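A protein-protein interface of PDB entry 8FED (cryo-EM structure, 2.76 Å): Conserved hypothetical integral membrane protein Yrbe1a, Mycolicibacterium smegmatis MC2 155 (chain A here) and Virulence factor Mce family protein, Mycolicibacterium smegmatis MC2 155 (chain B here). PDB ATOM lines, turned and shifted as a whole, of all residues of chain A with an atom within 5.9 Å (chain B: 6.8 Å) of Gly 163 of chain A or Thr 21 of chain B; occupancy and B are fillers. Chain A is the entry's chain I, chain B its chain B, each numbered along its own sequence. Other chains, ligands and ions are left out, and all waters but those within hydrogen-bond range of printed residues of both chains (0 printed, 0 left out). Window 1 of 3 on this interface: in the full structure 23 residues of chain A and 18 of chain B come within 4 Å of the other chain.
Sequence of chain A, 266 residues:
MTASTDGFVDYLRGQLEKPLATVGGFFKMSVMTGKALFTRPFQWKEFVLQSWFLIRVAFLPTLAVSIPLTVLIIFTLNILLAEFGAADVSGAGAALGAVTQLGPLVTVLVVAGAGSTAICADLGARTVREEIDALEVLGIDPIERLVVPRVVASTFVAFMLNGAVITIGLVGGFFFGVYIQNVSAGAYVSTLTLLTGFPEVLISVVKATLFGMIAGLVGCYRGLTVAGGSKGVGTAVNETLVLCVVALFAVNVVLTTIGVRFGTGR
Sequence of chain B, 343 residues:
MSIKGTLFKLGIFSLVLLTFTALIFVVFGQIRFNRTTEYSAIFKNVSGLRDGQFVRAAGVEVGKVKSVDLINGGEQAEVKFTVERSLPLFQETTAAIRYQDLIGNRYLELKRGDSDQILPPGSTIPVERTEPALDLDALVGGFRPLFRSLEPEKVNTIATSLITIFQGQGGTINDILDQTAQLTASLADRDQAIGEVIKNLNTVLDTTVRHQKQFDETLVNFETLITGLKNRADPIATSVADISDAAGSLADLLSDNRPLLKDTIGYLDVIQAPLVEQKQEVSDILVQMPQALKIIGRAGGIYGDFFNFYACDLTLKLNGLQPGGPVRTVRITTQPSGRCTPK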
ATOM      1  N   ALA A 158     -23.255  18.765  21.297  1.00  0.00           N
ATOM      2  CA  ALA A 158     -22.403  17.984  22.188  1.00  0.00           C
ATOM      3  C   ALA A 158     -22.704  16.495  22.071  1.00  0.00           C
ATOM      4  O   ALA A 158     -21.783  15.672  22.016  1.00  0.00           O
ATOM      5  CB  ALA A 158     -22.576  18.456  23.629  1.00  0.00           C
ATOM      6  N   PHE A 159     -23.989  16.137  22.023  1.00  0.00           N
ATOM      7  CA  PHE A 159     -24.382  14.739  21.851  1.00  0.00           C
ATOM      8  C   PHE A 159     -23.815  14.166  20.553  1.00  0.00           C
ATOM      9  O   PHE A 159     -23.152  13.112  20.550  1.00  0.00           O
ATOM     10  CB  PHE A 159     -25.911  14.654  21.877  1.00  0.00           C
ATOM     11  CG  PHE A 159     -26.462  13.265  21.733  1.00  0.00           C
ATOM     12  CD1 PHE A 159     -26.818  12.771  20.489  1.00  0.00           C
ATOM     13  CD2 PHE A 159     -26.662  12.469  22.845  1.00  0.00           C
ATOM     14  CE1 PHE A 159     -27.337  11.499  20.357  1.00  0.00           C
ATOM     15  CE2 PHE A 159     -27.182  11.198  22.717  1.00  0.00           C
ATOM     16  CZ  PHE A 159     -27.520  10.713  21.472  1.00  0.00           C
ATOM     17  N   MET A 160     -24.055  14.863  19.437  1.00  0.00           N
ATOM     18  CA  MET A 160     -23.593  14.374  18.141  1.00  0.00           C
ATOM     19  C   MET A 160     -22.072  14.270  18.089  1.00  0.00           C
ATOM     20  O   MET A 160     -21.523  13.280  17.582  1.00  0.00           O
ATOM     21  CB  MET A 160     -24.104  15.286  17.029  1.00  0.00           C
ATOM     22  CG  MET A 160     -25.575  15.119  16.720  1.00  0.00           C
ATOM     23  SD  MET A 160     -26.224  16.513  15.787  1.00  0.00           S
ATOM     24  CE  MET A 160     -24.913  16.785  14.605  1.00  0.00           C
ATOM     25  N   LEU A 161     -21.374  15.284  18.604  1.00  0.00           N
ATOM     26  CA  LEU A 161     -19.917  15.286  18.570  1.00  0.00           C
ATOM     27  C   LEU A 161     -19.342  14.188  19.449  1.00  0.00           C
ATOM     28  O   LEU A 161     -18.319  13.595  19.101  1.00  0.00           O
ATOM     29  CB  LEU A 161     -19.376  16.649  18.995  1.00  0.00           C
ATOM     30  CG  LEU A 161     -19.548  17.802  18.006  1.00  0.00           C
ATOM     31  CD1 LEU A 161     -18.870  19.049  18.539  1.00  0.00           C
ATOM     32  CD2 LEU A 161     -19.007  17.430  16.637  1.00  0.00           C
ATOM     33  N   ASN A 162     -19.970  13.905  20.594  1.00  0.00           N
ATOM     34  CA  ASN A 162     -19.509  12.803  21.431  1.00  0.00           C
ATOM     35  C   ASN A 162     -19.616  11.478  20.691  1.00  0.00           C
ATOM     36  O   ASN A 162     -18.678  10.665  20.705  1.00  0.00           O
ATOM     37  CB  ASN A 162     -20.316  12.759  22.726  1.00  0.00           C
ATOM     38  CG  ASN A 162     -20.096  11.483  23.511  1.00  0.00           C
ATOM     39  OD1 ASN A 162     -18.976  10.982  23.602  1.00  0.00           O
ATOM     40  ND2 ASN A 162     -21.168  10.947  24.078  1.00  0.00           N
ATOM     41  N   GLY A 163     -20.756  11.245  20.033  1.00  0.00           N
ATOM     42  CA  GLY A 163     -20.897  10.019  19.257  1.00  0.00           C
ATOM     43  C   GLY A 163     -19.845   9.901  18.169  1.00  0.00           C
ATOM     44  O   GLY A 163     -19.192   8.857  18.016  1.00  0.00           O
ATOM     45  N   ALA A 164     -19.650  10.985  17.410  1.00  0.00           N
ATOM     46  CA  ALA A 164     -18.670  10.970  16.328  1.00  0.00           C
ATOM     47  C   ALA A 164     -17.258  10.759  16.861  1.00  0.00           C
ATOM     48  O   ALA A 164     -16.463  10.033  16.256  1.00  0.00           O
ATOM     49  CB  ALA A 164     -18.751  12.266  15.526  1.00  0.00           C
ATOM     50  N   VAL A 165     -16.928  11.396  17.988  1.00  0.00           N
ATOM     51  CA  VAL A 165     -15.593  11.275  18.564  1.00  0.00           C
ATOM     52  C   VAL A 165     -15.324   9.840  18.987  1.00  0.00           C
ATOM     53  O   VAL A 165     -14.251   9.293  18.709  1.00  0.00           O
ATOM     54  CB  VAL A 165     -15.426  12.257  19.740  1.00  0.00           C
ATOM     55  CG1 VAL A 165     -14.299  11.815  20.657  1.00  0.00           C
ATOM     56  CG2 VAL A 165     -15.141  13.648  19.216  1.00  0.00           C
ATOM     57  N   ILE A 166     -16.293   9.203  19.651  1.00  0.00           N
ATOM     58  CA  ILE A 166     -16.100   7.815  20.071  1.00  0.00           C
ATOM     59  C   ILE A 166     -15.896   6.914  18.856  1.00  0.00           C
ATOM     60  O   ILE A 166     -14.976   6.082  18.827  1.00  0.00           O
ATOM     61  CB  ILE A 166     -17.280   7.342  20.938  1.00  0.00           C
ATOM     62  CG1 ILE A 166     -17.311   8.113  22.256  1.00  0.00           C
ATOM     63  CG2 ILE A 166     -17.169   5.855  21.214  1.00  0.00           C
ATOM     64  CD1 ILE A 166     -18.426   7.694  23.182  1.00  0.00           C
ATOM     65  N   THR A 167     -16.744   7.069  17.831  1.00  0.00           N
ATOM     66  CA  THR A 167     -16.633   6.208  16.653  1.00  0.00           C
ATOM     67  C   THR A 167     -15.289   6.389  15.950  1.00  0.00           C
ATOM     68  O   THR A 167     -14.601   5.407  15.632  1.00  0.00           O
ATOM     69  CB  THR A 167     -17.780   6.490  15.682  1.00  0.00           C
ATOM     70  OG1 THR A 167     -19.022   6.109  16.285  1.00  0.00           O
ATOM     71  CG2 THR A 167     -17.593   5.706  14.393  1.00  0.00           C
ATOM     72  N   ILE A 168     -14.897   7.643  15.705  1.00  0.00           N
ATOM     73  CA  ILE A 168     -13.653   7.913  14.992  1.00  0.00           C
ATOM     74  C   ILE A 168     -12.456   7.455  15.813  1.00  0.00           C
ATOM     75  O   ILE A 168     -11.482   6.924  15.266  1.00  0.00           O
ATOM     76  CB  ILE A 168     -13.564   9.406  14.621  1.00  0.00           C
ATOM     77  CG1 ILE A 168     -14.678   9.779  13.639  1.00  0.00           C
ATOM     78  CG2 ILE A 168     -12.207   9.744  14.021  1.00  0.00           C
ATOM     79  CD1 ILE A 168     -14.676   8.961  12.368  1.00  0.00           C
ATOM     80  N   VAL A 205     -23.427   9.180  27.099  1.00  0.00           N
ATOM     81  CA  VAL A 205     -24.462  10.063  26.565  1.00  0.00           C
ATOM     82  C   VAL A 205     -24.893  11.080  27.617  1.00  0.00           C
ATOM     83  O   VAL A 205     -25.063  12.272  27.321  1.00  0.00           O
ATOM     84  CB  VAL A 205     -25.649   9.229  26.051  1.00  0.00           C
ATOM     85  CG1 VAL A 205     -26.928  10.048  26.036  1.00  0.00           C
ATOM     86  CG2 VAL A 205     -25.348   8.684  24.664  1.00  0.00           C
ATOM     87  N   VAL B  16     -26.221  11.862   9.976  1.00  0.00           N
ATOM     88  CA  VAL B  16     -24.986  11.076   9.956  1.00  0.00           C
ATOM     89  C   VAL B  16     -24.484  10.817  11.375  1.00  0.00           C
ATOM     90  O   VAL B  16     -24.106   9.690  11.727  1.00  0.00           O
ATOM     91  CB  VAL B  16     -23.919  11.777   9.097  1.00  0.00           C
ATOM     92  CG1 VAL B  16     -22.588  11.056   9.210  1.00  0.00           C
ATOM     93  CG2 VAL B  16     -24.367  11.835   7.650  1.00  0.00           C
ATOM     94  N   LEU B  17     -24.478  11.850  12.220  1.00  0.00           N
ATOM     95  CA  LEU B  17     -23.916  11.666  13.555  1.00  0.00           C
ATOM     96  C   LEU B  17     -24.847  10.868  14.466  1.00  0.00           C
ATOM     97  O   LEU B  17     -24.370  10.112  15.323  1.00  0.00           O
ATOM     98  CB  LEU B  17     -23.556  13.020  14.163  1.00  0.00           C
ATOM     99  CG  LEU B  17     -22.466  13.770  13.382  1.00  0.00           C
ATOM    100  CD1 LEU B  17     -21.862  14.895  14.200  1.00  0.00           C
ATOM    101  CD2 LEU B  17     -21.370  12.828  12.902  1.00  0.00           C
ATOM    102  N   LEU B  18     -26.165  10.993  14.294  1.00  0.00           N
ATOM    103  CA  LEU B  18     -27.077  10.104  15.006  1.00  0.00           C
ATOM    104  C   LEU B  18     -26.953   8.671  14.510  1.00  0.00           C
ATOM    105  O   LEU B  18     -27.138   7.733  15.292  1.00  0.00           O
ATOM    106  CB  LEU B  18     -28.518  10.594  14.872  1.00  0.00           C
ATOM    107  CG  LEU B  18     -28.869  11.914  15.563  1.00  0.00           C
ATOM    108  CD1 LEU B  18     -30.325  12.276  15.320  1.00  0.00           C
ATOM    109  CD2 LEU B  18     -28.573  11.843  17.048  1.00  0.00           C
ATOM    110  N   THR B  19     -26.637   8.477  13.226  1.00  0.00           N
ATOM    111  CA  THR B  19     -26.335   7.138  12.735  1.00  0.00           C
ATOM    112  C   THR B  19     -25.097   6.576  13.419  1.00  0.00           C
ATOM    113  O   THR B  19     -25.062   5.397  13.783  1.00  0.00           O
ATOM    114  CB  THR B  19     -26.148   7.165  11.216  1.00  0.00           C
ATOM    115  OG1 THR B  19     -27.365   7.594  10.593  1.00  0.00           O
ATOM    116  CG2 THR B  19     -25.780   5.788  10.690  1.00  0.00           C
ATOM    117  N   PHE B  20     -24.073   7.412  13.610  1.00  0.00           N
ATOM    118  CA  PHE B  20     -22.885   6.971  14.341  1.00  0.00           C
ATOM    119  C   PHE B  20     -23.222   6.599  15.782  1.00  0.00           C
ATOM    120  O   PHE B  20     -22.740   5.582  16.299  1.00  0.00           O
ATOM    121  CB  PHE B  20     -21.811   8.057  14.315  1.00  0.00           C
ATOM    122  CG  PHE B  20     -20.963   8.043  13.078  1.00  0.00           C
ATOM    123  CD1 PHE B  20     -20.921   6.927  12.263  1.00  0.00           C
ATOM    124  CD2 PHE B  20     -20.205   9.149  12.732  1.00  0.00           C
ATOM    125  CE1 PHE B  20     -20.141   6.914  11.124  1.00  0.00           C
ATOM    126  CE2 PHE B  20     -19.424   9.141  11.594  1.00  0.00           C
ATOM    127  CZ  PHE B  20     -19.391   8.022  10.789  1.00  0.00           C
ATOM    128  N   THR B  21     -24.040   7.415  16.450  1.00  0.00           N
ATOM    129  CA  THR B  21     -24.428   7.110  17.826  1.00  0.00           C
ATOM    130  C   THR B  21     -25.232   5.814  17.905  1.00  0.00           C
ATOM    131  O   THR B  21     -25.017   4.989  18.803  1.00  0.00           O
ATOM    132  CB  THR B  21     -25.226   8.272  18.418  1.00  0.00           C
ATOM    133  OG1 THR B  21     -24.432   9.464  18.385  1.00  0.00           O
ATOM    134  CG2 THR B  21     -25.615   7.978  19.857  1.00  0.00           C
ATOM    135  N   ALA B  22     -26.163   5.614  16.968  1.00  0.00           N
ATOM    136  CA  ALA B  22     -26.939   4.380  16.938  1.00  0.00           C
ATOM    137  C   ALA B  22     -26.052   3.179  16.641  1.00  0.00           C
ATOM    138  O   ALA B  22     -26.281   2.087  17.171  1.00  0.00           O
ATOM    139  CB  ALA B  22     -28.060   4.489  15.907  1.00  0.00           C
ATOM    140  N   LEU B  23     -25.038   3.359  15.790  1.00  0.00           N
ATOM    141  CA  LEU B  23     -24.079   2.292  15.533  1.00  0.00           C
ATOM    142  C   LEU B  23     -23.314   1.932  16.796  1.00  0.00           C
ATOM    143  O   LEU B  23     -23.074   0.751  17.070  1.00  0.00           O
ATOM    144  CB  LEU B  23     -23.116   2.712  14.424  1.00  0.00           C
ATOM    145  CG  LEU B  23     -21.941   1.777  14.141  1.00  0.00           C
ATOM    146  CD1 LEU B  23     -22.437   0.416  13.675  1.00  0.00           C
ATOM    147  CD2 LEU B  23     -21.006   2.394  13.116  1.00  0.00           C
ATOM    148  N   ILE B  24     -22.919   2.940  17.577  1.00  0.00           N
ATOM    149  CA  ILE B  24     -22.262   2.686  18.857  1.00  0.00           C
ATOM    150  C   ILE B  24     -23.180   1.895  19.777  1.00  0.00           C
ATOM    151  O   ILE B  24     -22.756   0.932  20.430  1.00  0.00           O
ATOM    152  CB  ILE B  24     -21.826   4.013  19.506  1.00  0.00           C
ATOM    153  CG1 ILE B  24     -20.694   4.658  18.711  1.00  0.00           C
ATOM    154  CG2 ILE B  24     -21.393   3.796  20.943  1.00  0.00           C
ATOM    155  CD1 ILE B  24     -20.277   5.993  19.264  1.00  0.00           C
ATOM    156  N   PHE B  25     -24.454   2.294  19.847  1.00  0.00           N
ATOM    157  CA  PHE B  25     -25.407   1.592  20.704  1.00  0.00           C
ATOM    158  C   PHE B  25     -25.593   0.144  20.265  1.00  0.00           C
ATOM    159  O   PHE B  25     -25.647  -0.764  21.102  1.00  0.00           O
ATOM    160  CB  PHE B  25     -26.748   2.325  20.717  1.00  0.00           C
ATOM    161  CG  PHE B  25     -26.861   3.357  21.800  1.00  0.00           C
ATOM    162  CD1 PHE B  25     -27.270   3.000  23.073  1.00  0.00           C
ATOM    163  CD2 PHE B  25     -26.558   4.683  21.549  1.00  0.00           C
ATOM    164  CE1 PHE B  25     -27.374   3.944  24.074  1.00  0.00           C
ATOM    165  CE2 PHE B  25     -26.660   5.633  22.546  1.00  0.00           C
ATOM    166  CZ  PHE B  25     -27.069   5.262  23.810  1.00  0.00           C
ATOM    167  N   VAL B  26     -25.695  -0.090  18.955  1.00  0.00           N
ATOM    168  CA  VAL B  26     -25.858  -1.447  18.439  1.00  0.00           C
ATOM    169  C   VAL B  26     -24.621  -2.288  18.736  1.00  0.00           C
ATOM    170  O   VAL B  26     -24.727  -3.448  19.152  1.00  0.00           O
ATOM    171  CB  VAL B  26     -26.171  -1.409  16.931  1.00  0.00           C
ATOM    172  CG1 VAL B  26     -26.055  -2.794  16.321  1.00  0.00           C
ATOM    173  CG2 VAL B  26     -27.562  -0.846  16.696  1.00  0.00           C
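Hydrophobic or aromatic side chains of chain B that line the printed part of chain A: Leu 17, Leu 18, Phe 20, Ile 24 and Phe 25.
Along chain B the printed residues that touch a printed residue of chain A span positions 17 to 25.
Of the 12 printed residues of chain A, 7 touch a printed residue of chain B.
Hydrophobic or aromatic side chains of chain A within 4 Å of the printed part of chain B: Phe 159, Met 160, Ala 164, Ile 166 and Val 205.
Asn 162 of chain A touches none of the printed residues of chain B.
Of chain B, only Thr 21 and Ile 24 come within 4 Å of Gly 163 of chain A.
Printed residues of chain B within 4 Å of Ala 164 of chain A: Leu 17.
Of the printed residues of chain B, Ile 166 of chain A touches Ile 24 (3.7 Å).
Of the printed residues of chain B, Val 205 of chain A touches Phe 25 (3.9 Å).
Of the printed residues of chain A, Leu 18 of chain B touches Phe 159.
Of the printed residues of chain A, Thr 21 of chain B touches Phe 159 (3.7 Å) and Gly 163 (3.7 Å).
Of the printed residues of chain A, Phe 25 of chain B touches Val 205 (3.9 Å).
The nearest residue of chain B that does not touch Gly 163 of chain A is Phe 20 of chain B (4.6 Å).
The nearest printed residue of chain A that does not touch Leu 17 of chain B is Leu 161 of chain A (4.4 Å).
Phe 159 of chain A touches Leu 18 of chain B (CE1 to CD2, 3.5 Å).
Thr 21 of chain B touches Phe 159 of chain A (CG2 to CZ, 3.7 Å).
CE of Met 160 of chain A touches CD1 of Leu 17 of chain B, at 3.6 Å.
OG1 of Thr 21 of chain B touches CA of Gly 163 of chain A, 3.7 Å away.
O of Gly 163 of chain A touches CD1 of Ile 24 of chain B (3.3 Å).
CD2 of Leu 17 of chain B touches CB of Ala 164 of chain A, 3.7 Å away.
Ile 166 of chain A touches Ile 24 of chain B (CG2 to CD1, 3.7 Å).
Phe 20 of chain B touches Thr 167 of chain A (O to OG1, 3.8 Å).
Thr 167 of chain A touches Ile 24 of chain B.
CG2 of Val 205 of chain A touches CZ of Phe 25 of chain B (3.9 Å).
OG1 of Thr 21 of chain B sits at hydrogen-bond distance from O of Leu 17 of chain B, 3.1 Å away.
The backbone carbonyl oxygen (O) of Gly 163 of chain A lies within hydrogen-bond range of the side-chain hydroxyl (OG1) of Thr 167 of chain A (3.3 Å).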
